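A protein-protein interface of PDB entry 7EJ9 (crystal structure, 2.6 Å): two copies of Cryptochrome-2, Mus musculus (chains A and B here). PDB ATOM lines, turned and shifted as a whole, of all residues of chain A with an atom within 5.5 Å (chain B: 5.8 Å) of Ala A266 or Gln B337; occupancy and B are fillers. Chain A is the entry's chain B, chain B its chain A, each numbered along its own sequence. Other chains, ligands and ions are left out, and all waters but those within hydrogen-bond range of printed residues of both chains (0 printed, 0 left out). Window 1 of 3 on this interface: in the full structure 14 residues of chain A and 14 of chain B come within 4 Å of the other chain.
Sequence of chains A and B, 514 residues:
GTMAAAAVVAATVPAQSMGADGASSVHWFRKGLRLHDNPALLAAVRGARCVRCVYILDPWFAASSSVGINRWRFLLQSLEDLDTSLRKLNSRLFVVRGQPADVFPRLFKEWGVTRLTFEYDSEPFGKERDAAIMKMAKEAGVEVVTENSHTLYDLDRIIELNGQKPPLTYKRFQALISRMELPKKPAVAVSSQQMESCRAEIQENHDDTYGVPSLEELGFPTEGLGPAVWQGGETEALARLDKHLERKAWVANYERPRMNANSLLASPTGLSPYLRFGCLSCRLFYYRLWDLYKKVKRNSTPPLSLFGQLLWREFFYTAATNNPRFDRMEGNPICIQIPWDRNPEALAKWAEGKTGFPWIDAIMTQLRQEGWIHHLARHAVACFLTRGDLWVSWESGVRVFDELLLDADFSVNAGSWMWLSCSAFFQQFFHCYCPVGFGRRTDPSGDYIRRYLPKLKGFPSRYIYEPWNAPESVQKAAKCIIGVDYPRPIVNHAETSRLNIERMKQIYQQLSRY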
ATOM      1  N   VAL A 229      -0.272 -17.921  12.599  1.00  0.00           N
ATOM      2  CA  VAL A 229      -1.130 -17.381  11.551  1.00  0.00           C
ATOM      3  C   VAL A 229      -1.669 -16.012  11.951  1.00  0.00           C
ATOM      4  O   VAL A 229      -1.975 -15.174  11.092  1.00  0.00           O
ATOM      5  CB  VAL A 229      -2.256 -18.389  11.251  1.00  0.00           C
ATOM      6  CG1 VAL A 229      -3.349 -17.752  10.411  1.00  0.00           C
ATOM      7  CG2 VAL A 229      -1.674 -19.600  10.540  1.00  0.00           C
ATOM      8  N   TRP A 230      -1.764 -15.750  13.256  1.00  0.00           N
ATOM      9  CA  TRP A 230      -2.260 -14.483  13.798  1.00  0.00           C
ATOM     10  C   TRP A 230      -1.225 -13.968  14.806  1.00  0.00           C
ATOM     11  O   TRP A 230      -1.339 -14.213  16.012  1.00  0.00           O
ATOM     12  CB  TRP A 230      -3.641 -14.668  14.437  1.00  0.00           C
ATOM     13  CG  TRP A 230      -4.727 -15.112  13.492  1.00  0.00           C
ATOM     14  CD1 TRP A 230      -5.066 -16.398  13.166  1.00  0.00           C
ATOM     15  CD2 TRP A 230      -5.633 -14.265  12.771  1.00  0.00           C
ATOM     16  NE1 TRP A 230      -6.121 -16.400  12.279  1.00  0.00           N
ATOM     17  CE2 TRP A 230      -6.486 -15.105  12.021  1.00  0.00           C
ATOM     18  CE3 TRP A 230      -5.798 -12.880  12.681  1.00  0.00           C
ATOM     19  CZ2 TRP A 230      -7.497 -14.601  11.194  1.00  0.00           C
ATOM     20  CZ3 TRP A 230      -6.803 -12.378  11.860  1.00  0.00           C
ATOM     21  CH2 TRP A 230      -7.640 -13.239  11.129  1.00  0.00           C
ATOM     22  N   SER A 263     -13.298 -15.429   1.933  1.00  0.00           N
ATOM     23  CA  SER A 263     -12.543 -16.668   1.823  1.00  0.00           C
ATOM     24  C   SER A 263     -12.494 -17.338   3.189  1.00  0.00           C
ATOM     25  O   SER A 263     -12.640 -16.685   4.228  1.00  0.00           O
ATOM     26  CB  SER A 263     -11.112 -16.426   1.305  1.00  0.00           C
ATOM     27  N   LEU A 264     -12.298 -18.652   3.181  1.00  0.00           N
ATOM     28  CA  LEU A 264     -12.221 -19.377   4.439  1.00  0.00           C
ATOM     29  C   LEU A 264     -10.850 -19.280   5.093  1.00  0.00           C
ATOM     30  O   LEU A 264     -10.711 -19.661   6.258  1.00  0.00           O
ATOM     31  CB  LEU A 264     -12.606 -20.840   4.218  1.00  0.00           C
ATOM     32  CG  LEU A 264     -14.073 -21.019   3.812  1.00  0.00           C
ATOM     33  CD1 LEU A 264     -14.380 -22.474   3.503  1.00  0.00           C
ATOM     34  CD2 LEU A 264     -14.989 -20.486   4.908  1.00  0.00           C
ATOM     35  N   LEU A 265      -9.850 -18.762   4.394  1.00  0.00           N
ATOM     36  CA  LEU A 265      -8.506 -18.683   4.943  1.00  0.00           C
ATOM     37  C   LEU A 265      -8.322 -17.400   5.745  1.00  0.00           C
ATOM     38  O   LEU A 265      -8.995 -16.394   5.505  1.00  0.00           O
ATOM     39  CB  LEU A 265      -7.468 -18.758   3.824  1.00  0.00           C
ATOM     40  CG  LEU A 265      -7.533 -20.058   3.019  1.00  0.00           C
ATOM     41  CD1 LEU A 265      -6.438 -20.100   1.962  1.00  0.00           C
ATOM     42  CD2 LEU A 265      -7.440 -21.258   3.952  1.00  0.00           C
ATOM     43  N   ALA A 266      -7.394 -17.445   6.701  1.00  0.00           N
ATOM     44  CA  ALA A 266      -7.142 -16.297   7.566  1.00  0.00           C
ATOM     45  C   ALA A 266      -6.670 -15.091   6.765  1.00  0.00           C
ATOM     46  O   ALA A 266      -5.731 -15.186   5.969  1.00  0.00           O
ATOM     47  CB  ALA A 266      -6.104 -16.657   8.623  1.00  0.00           C
ATOM     48  N   SER A 267      -7.310 -13.953   6.995  1.00  0.00           N
ATOM     49  CA  SER A 267      -6.986 -12.733   6.263  1.00  0.00           C
ATOM     50  C   SER A 267      -5.800 -12.027   6.910  1.00  0.00           C
ATOM     51  O   SER A 267      -5.786 -11.848   8.132  1.00  0.00           O
ATOM     52  CB  SER A 267      -8.183 -11.795   6.229  1.00  0.00           C
ATOM     53  OG  SER A 267      -7.762 -10.444   6.127  1.00  0.00           O
ATOM     54  N   PRO A 268      -4.797 -11.607   6.134  1.00  0.00           N
ATOM     55  CA  PRO A 268      -3.697 -10.822   6.712  1.00  0.00           C
ATOM     56  C   PRO A 268      -4.085  -9.403   7.085  1.00  0.00           C
ATOM     57  O   PRO A 268      -3.231  -8.663   7.587  1.00  0.00           O
ATOM     58  CB  PRO A 268      -2.644 -10.825   5.597  1.00  0.00           C
ATOM     59  CG  PRO A 268      -3.430 -11.035   4.349  1.00  0.00           C
ATOM     60  CD  PRO A 268      -4.544 -11.960   4.726  1.00  0.00           C
ATOM     61  N   GLN A 366      -9.113 -26.337  11.461  1.00  0.00           N
ATOM     62  CA  GLN A 366      -8.586 -24.989  11.274  1.00  0.00           C
ATOM     63  C   GLN A 366      -8.692 -24.173  12.556  1.00  0.00           C
ATOM     64  O   GLN A 366      -7.754 -23.453  12.922  1.00  0.00           O
ATOM     65  CB  GLN A 366      -9.309 -24.280  10.128  1.00  0.00           C
ATOM     66  CG  GLN A 366      -8.795 -22.871   9.913  1.00  0.00           C
ATOM     67  CD  GLN A 366      -9.473 -22.157   8.763  1.00  0.00           C
ATOM     68  OE1 GLN A 366     -10.659 -22.359   8.497  1.00  0.00           O
ATOM     69  NE2 GLN A 366      -8.721 -21.313   8.076  1.00  0.00           N
ATOM     70  N   GLU A 370      -5.223 -22.860  13.977  1.00  0.00           N
ATOM     71  CA  GLU A 370      -4.906 -21.460  13.723  1.00  0.00           C
ATOM     72  C   GLU A 370      -5.505 -20.491  14.722  1.00  0.00           C
ATOM     73  O   GLU A 370      -4.924 -19.427  14.951  1.00  0.00           O
ATOM     74  CB  GLU A 370      -5.367 -21.058  12.318  1.00  0.00           C
ATOM     75  CG  GLU A 370      -4.484 -21.618  11.225  1.00  0.00           C
ATOM     76  CD  GLU A 370      -5.174 -21.663   9.888  1.00  0.00           C
ATOM     77  OE1 GLU A 370      -6.165 -20.915   9.711  1.00  0.00           O
ATOM     78  OE2 GLU A 370      -4.730 -22.456   9.025  1.00  0.00           O
ATOM     79  N   TRP A 372      -8.670 -19.167  14.393  1.00  0.00           N
ATOM     80  CA  TRP A 372      -9.743 -18.402  13.781  1.00  0.00           C
ATOM     81  C   TRP A 372     -10.405 -19.231  12.700  1.00  0.00           C
ATOM     82  O   TRP A 372      -9.737 -19.969  11.971  1.00  0.00           O
ATOM     83  CB  TRP A 372      -9.239 -17.087  13.184  1.00  0.00           C
ATOM     84  CG  TRP A 372     -10.295 -16.329  12.445  1.00  0.00           C
ATOM     85  CD1 TRP A 372     -11.120 -15.371  12.955  1.00  0.00           C
ATOM     86  CD2 TRP A 372     -10.648 -16.465  11.060  1.00  0.00           C
ATOM     87  NE1 TRP A 372     -11.964 -14.902  11.981  1.00  0.00           N
ATOM     88  CE2 TRP A 372     -11.695 -15.556  10.805  1.00  0.00           C
ATOM     89  CE3 TRP A 372     -10.180 -17.265  10.010  1.00  0.00           C
ATOM     90  CZ2 TRP A 372     -12.281 -15.424   9.543  1.00  0.00           C
ATOM     91  CZ3 TRP A 372     -10.767 -17.133   8.754  1.00  0.00           C
ATOM     92  CH2 TRP A 372     -11.804 -16.220   8.535  1.00  0.00           C
ATOM     93  N   MET B 329       2.885 -15.866   1.789  1.00  0.00           N
ATOM     94  CA  MET B 329       1.449 -15.674   1.582  1.00  0.00           C
ATOM     95  C   MET B 329       0.774 -15.247   2.881  1.00  0.00           C
ATOM     96  O   MET B 329       0.313 -14.108   3.009  1.00  0.00           O
ATOM     97  CB  MET B 329       0.801 -16.949   1.034  1.00  0.00           C
ATOM     98  CG  MET B 329      -0.689 -16.775   0.784  1.00  0.00           C
ATOM     99  SD  MET B 329      -1.576 -18.253   0.252  1.00  0.00           S
ATOM    100  CE  MET B 329      -1.657 -19.177   1.779  1.00  0.00           C
ATOM    101  N   GLU B 330       0.714 -16.156   3.852  1.00  0.00           N
ATOM    102  CA  GLU B 330       0.034 -15.878   5.110  1.00  0.00           C
ATOM    103  C   GLU B 330       0.636 -14.668   5.808  1.00  0.00           C
ATOM    104  O   GLU B 330       1.856 -14.496   5.851  1.00  0.00           O
ATOM    105  CB  GLU B 330       0.111 -17.087   6.039  1.00  0.00           C
ATOM    106  CG  GLU B 330      -0.830 -18.210   5.682  1.00  0.00           C
ATOM    107  CD  GLU B 330      -1.031 -19.162   6.845  1.00  0.00           C
ATOM    108  OE1 GLU B 330      -0.150 -19.190   7.731  1.00  0.00           O
ATOM    109  OE2 GLU B 330      -2.071 -19.864   6.887  1.00  0.00           O
ATOM    110  N   GLY B 331      -0.237 -13.832   6.368  1.00  0.00           N
ATOM    111  CA  GLY B 331       0.181 -12.651   7.089  1.00  0.00           C
ATOM    112  C   GLY B 331       0.623 -11.502   6.220  1.00  0.00           C
ATOM    113  O   GLY B 331       0.911 -10.423   6.754  1.00  0.00           O
ATOM    114  N   ASN B 332       0.673 -11.693   4.899  1.00  0.00           N
ATOM    115  CA  ASN B 332       1.157 -10.674   3.978  1.00  0.00           C
ATOM    116  C   ASN B 332      -0.017  -9.815   3.536  1.00  0.00           C
ATOM    117  O   ASN B 332      -0.858 -10.287   2.755  1.00  0.00           O
ATOM    118  CB  ASN B 332       1.825 -11.334   2.780  1.00  0.00           C
ATOM    119  CG  ASN B 332       2.381 -10.338   1.790  1.00  0.00           C
ATOM    120  OD1 ASN B 332       2.424  -9.136   2.051  1.00  0.00           O
ATOM    121  ND2 ASN B 332       2.813 -10.835   0.641  1.00  0.00           N
ATOM    122  N   CYS B 335      -1.207  -9.827  -0.175  1.00  0.00           N
ATOM    123  CA  CYS B 335      -1.282 -11.096  -0.886  1.00  0.00           C
ATOM    124  C   CYS B 335      -2.648 -11.746  -0.714  1.00  0.00           C
ATOM    125  O   CYS B 335      -3.198 -11.786   0.389  1.00  0.00           O
ATOM    126  CB  CYS B 335      -0.185 -12.052  -0.409  1.00  0.00           C
ATOM    127  SG  CYS B 335      -0.120 -13.588  -1.364  1.00  0.00           S
ATOM    128  N   ILE B 336      -3.197 -12.245  -1.819  1.00  0.00           N
ATOM    129  CA  ILE B 336      -4.429 -13.019  -1.754  1.00  0.00           C
ATOM    130  C   ILE B 336      -4.116 -14.389  -1.180  1.00  0.00           C
ATOM    131  O   ILE B 336      -3.124 -15.026  -1.557  1.00  0.00           O
ATOM    132  CB  ILE B 336      -5.074 -13.128  -3.145  1.00  0.00           C
ATOM    133  CG1 ILE B 336      -5.667 -11.785  -3.564  1.00  0.00           C
ATOM    134  CG2 ILE B 336      -6.134 -14.215  -3.173  1.00  0.00           C
ATOM    135  CD1 ILE B 336      -6.119 -11.765  -5.013  1.00  0.00           C
ATOM    136  N   GLN B 337      -4.954 -14.843  -0.253  1.00  0.00           N
ATOM    137  CA  GLN B 337      -4.739 -16.110   0.433  1.00  0.00           C
ATOM    138  C   GLN B 337      -5.427 -17.227  -0.343  1.00  0.00           C
ATOM    139  O   GLN B 337      -6.655 -17.233  -0.472  1.00  0.00           O
ATOM    140  CB  GLN B 337      -5.249 -16.022   1.870  1.00  0.00           C
ATOM    141  CG  GLN B 337      -4.703 -14.817   2.625  1.00  0.00           C
ATOM    142  CD  GLN B 337      -3.204 -14.895   2.831  1.00  0.00           C
ATOM    143  OE1 GLN B 337      -2.706 -15.843   3.436  1.00  0.00           O
ATOM    144  NE2 GLN B 337      -2.473 -13.910   2.318  1.00  0.00           N
ATOM    145  N   ILE B 338      -4.634 -18.168  -0.849  1.00  0.00           N
ATOM    146  CA  ILE B 338      -5.079 -19.203  -1.780  1.00  0.00           C
ATOM    147  C   ILE B 338      -4.609 -20.550  -1.251  1.00  0.00           C
ATOM    148  O   ILE B 338      -3.436 -20.682  -0.864  1.00  0.00           O
ATOM    149  CB  ILE B 338      -4.534 -18.939  -3.195  1.00  0.00           C
ATOM    150  CG1 ILE B 338      -5.102 -17.637  -3.756  1.00  0.00           C
ATOM    151  CG2 ILE B 338      -4.824 -20.110  -4.128  1.00  0.00           C
ATOM    152  CD1 ILE B 338      -4.379 -17.146  -4.992  1.00  0.00           C
ATOM    153  N   PRO B 339      -5.466 -21.574  -1.215  1.00  0.00           N
ATOM    154  CA  PRO B 339      -5.021 -22.877  -0.686  1.00  0.00           C
ATOM    155  C   PRO B 339      -4.204 -23.645  -1.719  1.00  0.00           C
ATOM    156  O   PRO B 339      -4.699 -24.478  -2.475  1.00  0.00           O
ATOM    157  CB  PRO B 339      -6.340 -23.584  -0.355  1.00  0.00           C
ATOM    158  CG  PRO B 339      -7.444 -22.717  -0.925  1.00  0.00           C
ATOM    159  CD  PRO B 339      -6.817 -21.661  -1.770  1.00  0.00           C
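Of the 9 printed residues of chain B, 6 touch a printed residue of chain A.
Printed residues of chain A that touch a printed residue of chain B: Val A229, Leu A265, Ala A266 and Pro A268.
Hydrophobic or aromatic side chains of chain A within 4 Å of the printed part of chain B: Val A229, Leu A265 and Pro A268.
Among the printed residues, 8 pairs touch across the chains.
Among the printed residues, no Asp or Glu carboxylate lies within 4 Å of a Lys or Arg side-chain nitrogen of the other chain.
No position is printed for both chains.
Among the printed residues, pairs that only touch across the chains: Pro A268 with Asn B332 (3.1 Å), Val A229 with Glu B330 (3.2 Å), Pro A268 with Gly B331 (3.4 Å), Ala A266 with Gln B337 (3.5 Å), Pro A268 with Gln B337 (3.5 Å), Leu A265 with Pro B339 (3.6 Å), Leu A265 with Ile B338 (3.7 Å) and Leu A265 with Gln B337 (3.8 Å).
Printed residues of chain B within 4 Å of Leu A265: Gln B337 (3.8 Å), Ile B338 (3.7 Å) and Pro B339 (3.6 Å).
Ala A266 touches just one residue of chain B: Gln B337.
Ser A267 touches none of the printed residues of chain B.
Of the printed residues of chain A, Glu B330 touches Val A229 (3.2 Å).
Printed residues of chain A within 4 Å of Gly B331: Pro A268.
Of the printed residues of chain A, Asn B332 touches Pro A268.
Ile B336 touches none of the printed residues of chain A.
Of the printed residues of chain A, Pro B339 touches Leu A265.
The nearest residue of chain B that does not touch Ala A266 is Glu B330 (5.4 Å).
The nearest residue of chain A that does not touch Gln B337 is Ser A267 (4.8 Å).
The backbone NH (N) of Ile B338 is in hydrogen-bond range of the side-chain sulfur (SD) of Met B329 (3.3 Å).
The backbone NH of Glu B330 sits close to the side-chain amide oxygen of Gln B337.
O of Met B329 lies within hydrogen-bond range of NE2 of Gln B337.
The side-chain amide nitrogen (NE2) of Gln B337 sits at hydrogen-bond distance from the backbone carbonyl oxygen (O) of Cys B335 (3.0 Å).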
